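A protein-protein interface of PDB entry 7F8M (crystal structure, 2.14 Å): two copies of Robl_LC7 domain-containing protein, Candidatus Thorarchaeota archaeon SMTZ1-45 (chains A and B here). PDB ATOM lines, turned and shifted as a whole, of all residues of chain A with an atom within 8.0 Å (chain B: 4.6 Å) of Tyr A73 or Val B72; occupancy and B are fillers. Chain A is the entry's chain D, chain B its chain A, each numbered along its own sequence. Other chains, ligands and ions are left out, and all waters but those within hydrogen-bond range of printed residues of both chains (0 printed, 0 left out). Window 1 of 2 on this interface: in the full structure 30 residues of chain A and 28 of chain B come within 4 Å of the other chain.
Printed residues of chain A that touch a printed residue of chain B: Gly A57, Ala A60, Glu A71, Val A72, Tyr A73, Val A74, Lys A75 and Phe A106. Hydrophobic or aromatic side chains of chain A within 4 Å of the printed part of chain B: Ala A60, Val A72, Tyr A73, Val A74 and Phe A106. Among the printed residues, 13 pairs touch across the chains. Among the printed residues, no Asp or Glu carboxylate lies within 4 Å of a Lys or Arg side-chain nitrogen of the other chain.
The side-chain carboxylate (OE1) of Glu B71 is in hydrogen-bond range of the side-chain hydroxyl (OH) of Tyr A73 (2.9 Å). The backbone carbonyl oxygen (O) of Glu B71 lies within hydrogen-bond range of the backbone NH (N) of Lys A75 (3.0 Å). N of Tyr A73 is in hydrogen-bond range of O of Tyr B73, 2.8 Å away.
N of Val B72 is in hydrogen-bond range of O of Leu B83, 2.8 Å away. N of Val B74 sits at hydrogen-bond distance from O of Thr B81 (3.0 Å). The backbone NH (N) of Val A72 is in hydrogen-bond range of the backbone carbonyl oxygen (O) of Leu A83 (3.2 Å). The backbone carbonyl oxygen (O) of Val A74 sits at hydrogen-bond distance from the backbone NH (N) of Thr A81 (3.0 Å).
O of Gly A57 touches CG1 of Val B74 (3.8 Å). Ala A60 touches Leu B53. O of Glu A71 touches CA of Val B74, 3.7 Å away. Val A72 touches Tyr B73 (CA to O, 3.6 Å). CG2 of Val B72 touches O of Tyr A73, at 3.3 Å. Val A74 touches Phe B69. Glu B71 touches Val A74 (O to CA, 3.6 Å). Val A74 touches Val B72. O of Lys A75 touches C of Phe B69, 3.8 Å away. OH of Tyr B73 touches CE2 of Phe A106, 3.0 Å away.
Val A72 touches Tyr B73, and with the chains exchanged Tyr A73 touches Val B72. Tyr A73 touches Glu B71, but with the chains exchanged Glu A71 does not touch Tyr B73 (4.1 Å). Val A74 touches Val B72, but with the chains exchanged Val A72 does not touch Val B74 (4.01 Å). Phe A106 touches Tyr B73, but with the chains exchanged Tyr A73 does not touch Phe B106 (4.4 Å). 10 positions are printed for both chains.
Of the printed residues of chain B, Ala A60 touches Leu B53. Printed residues of chain B within 4 Å of Val A72: Tyr B73. Tyr A73 touches three residues of chain B. Printed residues of chain B within 4 Å of Lys A75: Phe B69 (3.8 Å) and Glu B71 (3.0 Å). Printed residues of chain A within 4 Å of Glu B71: Tyr A73, Val A74 and Lys A75. Of chain A, only Tyr A73 (3.3 Å) and Val A74 (3.9 Å) come within 4 Å of Val B72. The nearest residue of chain B that does not touch Tyr A73 is Phe B106 (4.4 Å). The nearest printed residue of chain A that does not touch Glu B71 is Gly A76 (5.5 Å).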
ATOM      1  N   LEU A  53      28.964 -17.564  21.302  1.00  0.00           N
ATOM      2  CA  LEU A  53      27.909 -17.202  20.312  1.00  0.00           C
ATOM      3  C   LEU A  53      27.487 -18.414  19.462  1.00  0.00           C
ATOM      4  O   LEU A  53      26.268 -18.491  19.079  1.00  0.00           O
ATOM      5  CB  LEU A  53      28.437 -16.087  19.404  1.00  0.00           C
ATOM      6  CG  LEU A  53      28.724 -14.747  20.094  1.00  0.00           C
ATOM      7  CD1 LEU A  53      28.744 -13.644  19.021  1.00  0.00           C
ATOM      8  CD2 LEU A  53      27.695 -14.443  21.194  1.00  0.00           C
ATOM      9  N   LEU A  56      25.822 -21.205  22.278  1.00  0.00           N
ATOM     10  CA  LEU A  56      24.514 -20.593  22.654  1.00  0.00           C
ATOM     11  C   LEU A  56      23.674 -20.236  21.408  1.00  0.00           C
ATOM     12  O   LEU A  56      22.497 -19.882  21.576  1.00  0.00           O
ATOM     13  CB  LEU A  56      24.749 -19.352  23.518  1.00  0.00           C
ATOM     14  CG  LEU A  56      25.780 -19.484  24.634  1.00  0.00           C
ATOM     15  CD1 LEU A  56      26.197 -18.090  25.099  1.00  0.00           C
ATOM     16  CD2 LEU A  56      25.250 -20.352  25.794  1.00  0.00           C
ATOM     17  N   GLY A  57      24.240 -20.299  20.203  1.00  0.00           N
ATOM     18  CA  GLY A  57      23.496 -20.297  18.923  1.00  0.00           C
ATOM     19  C   GLY A  57      23.075 -21.719  18.539  1.00  0.00           C
ATOM     20  O   GLY A  57      22.023 -21.914  17.926  1.00  0.00           O
ATOM     21  N   ALA A  60      19.610 -22.636  20.694  1.00  0.00           N
ATOM     22  CA  ALA A  60      18.279 -22.291  20.142  1.00  0.00           C
ATOM     23  C   ALA A  60      17.935 -23.195  18.958  1.00  0.00           C
ATOM     24  O   ALA A  60      16.754 -23.508  18.801  1.00  0.00           O
ATOM     25  CB  ALA A  60      18.189 -20.857  19.711  1.00  0.00           C
ATOM     26  N   PHE A  69      22.615 -25.849  12.860  1.00  0.00           N
ATOM     27  CA  PHE A  69      23.048 -24.428  12.993  1.00  0.00           C
ATOM     28  C   PHE A  69      23.674 -23.998  11.660  1.00  0.00           C
ATOM     29  O   PHE A  69      24.497 -24.747  11.141  1.00  0.00           O
ATOM     30  CB  PHE A  69      24.017 -24.202  14.175  1.00  0.00           C
ATOM     31  CG  PHE A  69      24.510 -22.774  14.320  1.00  0.00           C
ATOM     32  CD1 PHE A  69      23.671 -21.770  14.799  1.00  0.00           C
ATOM     33  CD2 PHE A  69      25.783 -22.403  13.890  1.00  0.00           C
ATOM     34  CE1 PHE A  69      24.116 -20.457  14.892  1.00  0.00           C
ATOM     35  CE2 PHE A  69      26.197 -21.076  13.933  1.00  0.00           C
ATOM     36  CZ  PHE A  69      25.360 -20.105  14.433  1.00  0.00           C
ATOM     37  N   GLU A  71      23.759 -19.971  10.960  1.00  0.00           N
ATOM     38  CA  GLU A  71      24.058 -18.519  11.018  1.00  0.00           C
ATOM     39  C   GLU A  71      23.415 -17.883  12.247  1.00  0.00           C
ATOM     40  O   GLU A  71      22.312 -18.284  12.634  1.00  0.00           O
ATOM     41  CB  GLU A  71      23.470 -17.762   9.813  1.00  0.00           C
ATOM     42  CG  GLU A  71      23.931 -18.213   8.444  1.00  0.00           C
ATOM     43  CD  GLU A  71      23.457 -17.351   7.260  1.00  0.00           C
ATOM     44  OE1 GLU A  71      22.392 -16.646   7.393  1.00  0.00           O
ATOM     45  OE2 GLU A  71      24.184 -17.354   6.188  1.00  0.00           O
ATOM     46  N   VAL A  72      24.054 -16.859  12.782  1.00  0.00           N
ATOM     47  CA  VAL A  72      23.559 -16.123  13.963  1.00  0.00           C
ATOM     48  C   VAL A  72      23.780 -14.638  13.697  1.00  0.00           C
ATOM     49  O   VAL A  72      24.849 -14.251  13.167  1.00  0.00           O
ATOM     50  CB  VAL A  72      24.241 -16.597  15.256  1.00  0.00           C
ATOM     51  CG1 VAL A  72      25.704 -16.214  15.305  1.00  0.00           C
ATOM     52  CG2 VAL A  72      23.535 -16.096  16.478  1.00  0.00           C
ATOM     53  N   TYR A  73      22.772 -13.844  13.997  1.00  0.00           N
ATOM     54  CA  TYR A  73      22.749 -12.361  13.826  1.00  0.00           C
ATOM     55  C   TYR A  73      22.460 -11.789  15.224  1.00  0.00           C
ATOM     56  O   TYR A  73      21.510 -12.248  15.854  1.00  0.00           O
ATOM     57  CB  TYR A  73      21.838 -12.009  12.632  1.00  0.00           C
ATOM     58  CG  TYR A  73      21.236 -10.609  12.508  1.00  0.00           C
ATOM     59  CD1 TYR A  73      21.602  -9.725  11.519  1.00  0.00           C
ATOM     60  CD2 TYR A  73      20.198 -10.209  13.330  1.00  0.00           C
ATOM     61  CE1 TYR A  73      21.023  -8.457  11.399  1.00  0.00           C
ATOM     62  CE2 TYR A  73      19.631  -8.956  13.252  1.00  0.00           C
ATOM     63  CZ  TYR A  73      20.017  -8.077  12.269  1.00  0.00           C
ATOM     64  OH  TYR A  73      19.406  -6.857  12.278  1.00  0.00           O
ATOM     65  N   VAL A  74      23.337 -10.919  15.744  1.00  0.00           N
ATOM     66  CA  VAL A  74      22.936  -9.932  16.798  1.00  0.00           C
ATOM     67  C   VAL A  74      23.151  -8.473  16.367  1.00  0.00           C
ATOM     68  O   VAL A  74      24.184  -8.169  15.636  1.00  0.00           O
ATOM     69  CB  VAL A  74      23.689 -10.234  18.100  1.00  0.00           C
ATOM     70  CG1 VAL A  74      23.118  -9.440  19.261  1.00  0.00           C
ATOM     71  CG2 VAL A  74      23.655 -11.716  18.476  1.00  0.00           C
ATOM     72  N   LYS A  75      22.269  -7.568  16.782  1.00  0.00           N
ATOM     73  CA  LYS A  75      22.352  -6.100  16.446  1.00  0.00           C
ATOM     74  C   LYS A  75      22.253  -5.245  17.719  1.00  0.00           C
ATOM     75  O   LYS A  75      21.360  -5.468  18.598  1.00  0.00           O
ATOM     76  CB  LYS A  75      21.283  -5.628  15.447  1.00  0.00           C
ATOM     77  CG  LYS A  75      21.371  -4.138  15.038  1.00  0.00           C
ATOM     78  CD  LYS A  75      20.164  -3.613  14.293  1.00  0.00           C
ATOM     79  CE  LYS A  75      20.250  -2.191  13.781  1.00  0.00           C
ATOM     80  NZ  LYS A  75      18.933  -1.731  13.291  1.00  0.00           N
ATOM     81  N   GLY A  76      23.202  -4.339  17.867  1.00  0.00           N
ATOM     82  CA  GLY A  76      23.228  -3.333  18.941  1.00  0.00           C
ATOM     83  C   GLY A  76      23.132  -1.943  18.309  1.00  0.00           C
ATOM     84  O   GLY A  76      23.431  -1.791  17.098  1.00  0.00           O
ATOM     85  N   GLY A  79      26.193  -0.893  16.334  1.00  0.00           N
ATOM     86  CA  GLY A  79      26.698  -1.794  15.273  1.00  0.00           C
ATOM     87  C   GLY A  79      26.235  -3.229  15.457  1.00  0.00           C
ATOM     88  O   GLY A  79      25.380  -3.465  16.329  1.00  0.00           O
ATOM     89  N   TYR A  80      26.782  -4.147  14.644  1.00  0.00           N
ATOM     90  CA  TYR A  80      26.291  -5.539  14.494  1.00  0.00           C
ATOM     91  C   TYR A  80      27.443  -6.535  14.697  1.00  0.00           C
ATOM     92  O   TYR A  80      28.591  -6.358  14.197  1.00  0.00           O
ATOM     93  CB  TYR A  80      25.702  -5.860  13.114  1.00  0.00           C
ATOM     94  CG  TYR A  80      24.514  -5.074  12.583  1.00  0.00           C
ATOM     95  CD1 TYR A  80      23.249  -5.631  12.486  1.00  0.00           C
ATOM     96  CD2 TYR A  80      24.702  -3.845  11.971  1.00  0.00           C
ATOM     97  CE1 TYR A  80      22.171  -4.934  11.939  1.00  0.00           C
ATOM     98  CE2 TYR A  80      23.652  -3.153  11.395  1.00  0.00           C
ATOM     99  CZ  TYR A  80      22.375  -3.685  11.375  1.00  0.00           C
ATOM    100  OH  TYR A  80      21.399  -2.923  10.765  1.00  0.00           O
ATOM    101  N   THR A  81      27.100  -7.661  15.306  1.00  0.00           N
ATOM    102  CA  THR A  81      27.934  -8.864  15.329  1.00  0.00           C
ATOM    103  C   THR A  81      27.329  -9.951  14.442  1.00  0.00           C
ATOM    104  O   THR A  81      26.240 -10.452  14.717  1.00  0.00           O
ATOM    105  CB  THR A  81      28.070  -9.338  16.773  1.00  0.00           C
ATOM    106  OG1 THR A  81      28.698  -8.345  17.587  1.00  0.00           O
ATOM    107  CG2 THR A  81      28.921 -10.578  16.837  1.00  0.00           C
ATOM    108  N   LEU A  82      28.071 -10.406  13.464  1.00  0.00           N
ATOM    109  CA  LEU A  82      27.621 -11.489  12.568  1.00  0.00           C
ATOM    110  C   LEU A  82      28.580 -12.650  12.714  1.00  0.00           C
ATOM    111  O   LEU A  82      29.803 -12.350  12.892  1.00  0.00           O
ATOM    112  CB  LEU A  82      27.662 -10.989  11.122  1.00  0.00           C
ATOM    113  CG  LEU A  82      26.856  -9.737  10.815  1.00  0.00           C
ATOM    114  CD1 LEU A  82      26.977  -9.423   9.353  1.00  0.00           C
ATOM    115  CD2 LEU A  82      25.378  -9.851  11.200  1.00  0.00           C
ATOM    116  N   LEU A  83      28.038 -13.878  12.650  1.00  0.00           N
ATOM    117  CA  LEU A  83      28.836 -15.143  12.656  1.00  0.00           C
ATOM    118  C   LEU A  83      28.199 -16.173  11.713  1.00  0.00           C
ATOM    119  O   LEU A  83      26.992 -16.323  11.771  1.00  0.00           O
ATOM    120  CB  LEU A  83      28.849 -15.643  14.102  1.00  0.00           C
ATOM    121  CG  LEU A  83      29.783 -16.808  14.434  1.00  0.00           C
ATOM    122  CD1 LEU A  83      30.120 -16.778  15.917  1.00  0.00           C
ATOM    123  CD2 LEU A  83      29.142 -18.171  14.090  1.00  0.00           C
ATOM    124  N   THR A  84      29.012 -16.895  10.959  1.00  0.00           N
ATOM    125  CA  THR A  84      28.616 -18.006  10.042  1.00  0.00           C
ATOM    126  C   THR A  84      29.535 -19.208  10.283  1.00  0.00           C
ATOM    127  O   THR A  84      30.703 -18.999  10.612  1.00  0.00           O
ATOM    128  CB  THR A  84      28.650 -17.652   8.527  1.00  0.00           C
ATOM    129  OG1 THR A  84      29.921 -17.372   7.910  1.00  0.00           O
ATOM    130  CG2 THR A  84      27.745 -16.485   8.212  1.00  0.00           C
ATOM    131  N   ALA A 100      25.501  -0.629   7.977  1.00  0.00           N
ATOM    132  CA  ALA A 100      25.973  -1.501   6.868  1.00  0.00           C
ATOM    133  C   ALA A 100      24.787  -2.346   6.389  1.00  0.00           C
ATOM    134  O   ALA A 100      23.762  -2.394   7.113  1.00  0.00           O
ATOM    135  CB  ALA A 100      27.164  -2.321   7.279  1.00  0.00           C
ATOM    136  N   ILE A 102      23.379  -5.830   5.628  1.00  0.00           N
ATOM    137  CA  ILE A 102      23.663  -7.144   6.288  1.00  0.00           C
ATOM    138  C   ILE A 102      23.460  -8.264   5.270  1.00  0.00           C
ATOM    139  O   ILE A 102      24.267  -9.255   5.225  1.00  0.00           O
ATOM    140  CB  ILE A 102      22.711  -7.276   7.516  1.00  0.00           C
ATOM    141  CG1 ILE A 102      23.009  -6.190   8.552  1.00  0.00           C
ATOM    142  CG2 ILE A 102      22.689  -8.669   8.132  1.00  0.00           C
ATOM    143  CD1 ILE A 102      24.441  -6.155   9.007  1.00  0.00           C
ATOM    144  N   GLY A 103      22.372  -8.165   4.520  1.00  0.00           N
ATOM    145  CA  GLY A 103      21.964  -9.211   3.556  1.00  0.00           C
ATOM    146  C   GLY A 103      23.049  -9.484   2.520  1.00  0.00           C
ATOM    147  O   GLY A 103      23.219 -10.663   2.110  1.00  0.00           O
ATOM    148  N   PHE A 106      26.302 -11.197   4.401  1.00  0.00           N
ATOM    149  CA  PHE A 106      26.030 -12.646   4.572  1.00  0.00           C
ATOM    150  C   PHE A 106      26.315 -13.363   3.246  1.00  0.00           C
ATOM    151  O   PHE A 106      26.937 -14.421   3.253  1.00  0.00           O
ATOM    152  CB  PHE A 106      24.634 -12.889   5.176  1.00  0.00           C
ATOM    153  CG  PHE A 106      24.565 -13.010   6.692  1.00  0.00           C
ATOM    154  CD1 PHE A 106      25.509 -13.729   7.408  1.00  0.00           C
ATOM    155  CD2 PHE A 106      23.500 -12.466   7.401  1.00  0.00           C
ATOM    156  CE1 PHE A 106      25.450 -13.837   8.796  1.00  0.00           C
ATOM    157  CE2 PHE A 106      23.410 -12.618   8.780  1.00  0.00           C
ATOM    158  CZ  PHE A 106      24.389 -13.291   9.478  1.00  0.00           C
ATOM    159  N   LEU B  53      17.771 -16.695  25.120  1.00  0.00           N
ATOM    160  CA  LEU B  53      18.264 -16.037  23.865  1.00  0.00           C
ATOM    161  C   LEU B  53      18.428 -14.537  24.034  1.00  0.00           C
ATOM    162  O   LEU B  53      19.160 -13.933  23.161  1.00  0.00           O
ATOM    163  CB  LEU B  53      17.276 -16.233  22.705  1.00  0.00           C
ATOM    164  CG  LEU B  53      17.578 -17.443  21.830  1.00  0.00           C
ATOM    165  CD1 LEU B  53      17.523 -18.720  22.687  1.00  0.00           C
ATOM    166  CD2 LEU B  53      16.636 -17.483  20.625  1.00  0.00           C
ATOM    167  N   PHE B  69      21.599  -3.516  23.277  1.00  0.00           N
ATOM    168  CA  PHE B  69      21.006  -4.654  22.516  1.00  0.00           C
ATOM    169  C   PHE B  69      19.745  -4.207  21.776  1.00  0.00           C
ATOM    170  O   PHE B  69      18.964  -3.433  22.354  1.00  0.00           O
ATOM    171  CB  PHE B  69      20.565  -5.792  23.431  1.00  0.00           C
ATOM    172  CG  PHE B  69      19.786  -6.865  22.711  1.00  0.00           C
ATOM    173  CD1 PHE B  69      20.447  -7.788  21.895  1.00  0.00           C
ATOM    174  CD2 PHE B  69      18.402  -6.923  22.793  1.00  0.00           C
ATOM    175  CE1 PHE B  69      19.736  -8.756  21.194  1.00  0.00           C
ATOM    176  CE2 PHE B  69      17.704  -7.906  22.103  1.00  0.00           C
ATOM    177  CZ  PHE B  69      18.375  -8.829  21.334  1.00  0.00           C
ATOM    178  N   GLU B  71      18.225  -6.545  18.608  1.00  0.00           N
ATOM    179  CA  GLU B  71      17.572  -7.676  17.895  1.00  0.00           C
ATOM    180  C   GLU B  71      18.502  -8.884  17.875  1.00  0.00           C
ATOM    181  O   GLU B  71      19.733  -8.717  17.877  1.00  0.00           O
ATOM    182  CB  GLU B  71      17.311  -7.314  16.429  1.00  0.00           C
ATOM    183  CG  GLU B  71      16.628  -5.979  16.197  1.00  0.00           C
ATOM    184  CD  GLU B  71      16.396  -5.668  14.718  1.00  0.00           C
ATOM    185  OE1 GLU B  71      17.080  -6.306  13.866  1.00  0.00           O
ATOM    186  OE2 GLU B  71      15.458  -4.870  14.425  1.00  0.00           O
ATOM    187  N   VAL B  72      17.947 -10.074  17.737  1.00  0.00           N
ATOM    188  CA  VAL B  72      18.811 -11.253  17.455  1.00  0.00           C
ATOM    189  C   VAL B  72      18.007 -12.270  16.635  1.00  0.00           C
ATOM    190  O   VAL B  72      16.798 -12.429  16.860  1.00  0.00           O
ATOM    191  CB  VAL B  72      19.380 -11.808  18.772  1.00  0.00           C
ATOM    192  CG1 VAL B  72      18.356 -11.854  19.869  1.00  0.00           C
ATOM    193  CG2 VAL B  72      19.995 -13.171  18.597  1.00  0.00           C
ATOM    194  N   TYR B  73      18.641 -12.912  15.666  1.00  0.00           N
ATOM    195  CA  TYR B  73      18.027 -14.041  14.926  1.00  0.00           C
ATOM    196  C   TYR B  73      19.029 -15.169  14.735  1.00  0.00           C
ATOM    197  O   TYR B  73      20.230 -14.914  14.580  1.00  0.00           O
ATOM    198  CB  TYR B  73      17.460 -13.613  13.570  1.00  0.00           C
ATOM    199  CG  TYR B  73      18.361 -13.562  12.350  1.00  0.00           C
ATOM    200  CD1 TYR B  73      18.903 -14.700  11.756  1.00  0.00           C
ATOM    201  CD2 TYR B  73      18.449 -12.379  11.637  1.00  0.00           C
ATOM    202  CE1 TYR B  73      19.643 -14.634  10.571  1.00  0.00           C
ATOM    203  CE2 TYR B  73      19.155 -12.286  10.443  1.00  0.00           C
ATOM    204  CZ  TYR B  73      19.763 -13.420   9.913  1.00  0.00           C
ATOM    205  OH  TYR B  73      20.445 -13.308   8.737  1.00  0.00           O
ATOM    206  N   VAL B  74      18.506 -16.394  14.803  1.00  0.00           N
ATOM    207  CA  VAL B  74      19.255 -17.641  14.535  1.00  0.00           C
ATOM    208  C   VAL B  74      18.624 -18.395  13.373  1.00  0.00           C
ATOM    209  O   VAL B  74      17.435 -18.732  13.394  1.00  0.00           O
ATOM    210  CB  VAL B  74      19.261 -18.516  15.776  1.00  0.00           C
ATOM    211  CG1 VAL B  74      19.923 -19.845  15.474  1.00  0.00           C
ATOM    212  CG2 VAL B  74      19.940 -17.813  16.938  1.00  0.00           C
ATOM    213  N   THR B  81      14.490 -18.413  14.166  1.00  0.00           N
ATOM    214  CA  THR B  81      13.978 -17.784  15.403  1.00  0.00           C
ATOM    215  C   THR B  81      14.377 -16.302  15.454  1.00  0.00           C
ATOM    216  O   THR B  81      15.580 -16.053  15.397  1.00  0.00           O
ATOM    217  CB  THR B  81      14.540 -18.526  16.613  1.00  0.00           C
ATOM    218  OG1 THR B  81      14.608 -19.914  16.276  1.00  0.00           O
ATOM    219  CG2 THR B  81      13.687 -18.263  17.835  1.00  0.00           C
ATOM    220  N   LEU B  82      13.435 -15.388  15.697  1.00  0.00           N
ATOM    221  CA  LEU B  82      13.589 -13.921  15.503  1.00  0.00           C
ATOM    222  C   LEU B  82      13.159 -13.243  16.809  1.00  0.00           C
ATOM    223  O   LEU B  82      12.065 -13.659  17.321  1.00  0.00           O
ATOM    224  CB  LEU B  82      12.724 -13.426  14.341  1.00  0.00           C
ATOM    225  CG  LEU B  82      12.733 -14.227  13.019  1.00  0.00           C
ATOM    226  CD1 LEU B  82      11.746 -13.642  11.988  1.00  0.00           C
ATOM    227  CD2 LEU B  82      14.077 -14.280  12.335  1.00  0.00           C
ATOM    228  N   LEU B  83      14.000 -12.326  17.342  1.00  0.00           N
ATOM    229  CA  LEU B  83      13.753 -11.723  18.666  1.00  0.00           C
ATOM    230  C   LEU B  83      14.125 -10.256  18.654  1.00  0.00           C
ATOM    231  O   LEU B  83      15.219  -9.906  18.284  1.00  0.00           O
ATOM    232  CB  LEU B  83      14.565 -12.499  19.722  1.00  0.00           C
ATOM    233  CG  LEU B  83      14.247 -12.172  21.176  1.00  0.00           C
ATOM    234  CD1 LEU B  83      14.780 -13.274  22.105  1.00  0.00           C
ATOM    235  CD2 LEU B  83      14.855 -10.825  21.578  1.00  0.00           C
ATOM    236  N   PHE B 106      11.568  -7.712  10.593  1.00  0.00           N
ATOM    237  CA  PHE B 106      12.295  -6.883  11.592  1.00  0.00           C
ATOM    238  C   PHE B 106      11.832  -5.426  11.576  1.00  0.00           C
ATOM    239  O   PHE B 106      11.788  -4.751  12.672  1.00  0.00           O
ATOM    240  CB  PHE B 106      13.810  -7.016  11.414  1.00  0.00           C
ATOM    241  CG  PHE B 106      14.355  -8.214  12.156  1.00  0.00           C
ATOM    242  CD1 PHE B 106      14.196  -8.315  13.527  1.00  0.00           C
ATOM    243  CD2 PHE B 106      15.046  -9.211  11.483  1.00  0.00           C
ATOM    244  CE1 PHE B 106      14.743  -9.375  14.243  1.00  0.00           C
ATOM    245  CE2 PHE B 106      15.549 -10.297  12.182  1.00  0.00           C
ATOM    246  CZ  PHE B 106      15.376 -10.384  13.551  1.00  0.00           C
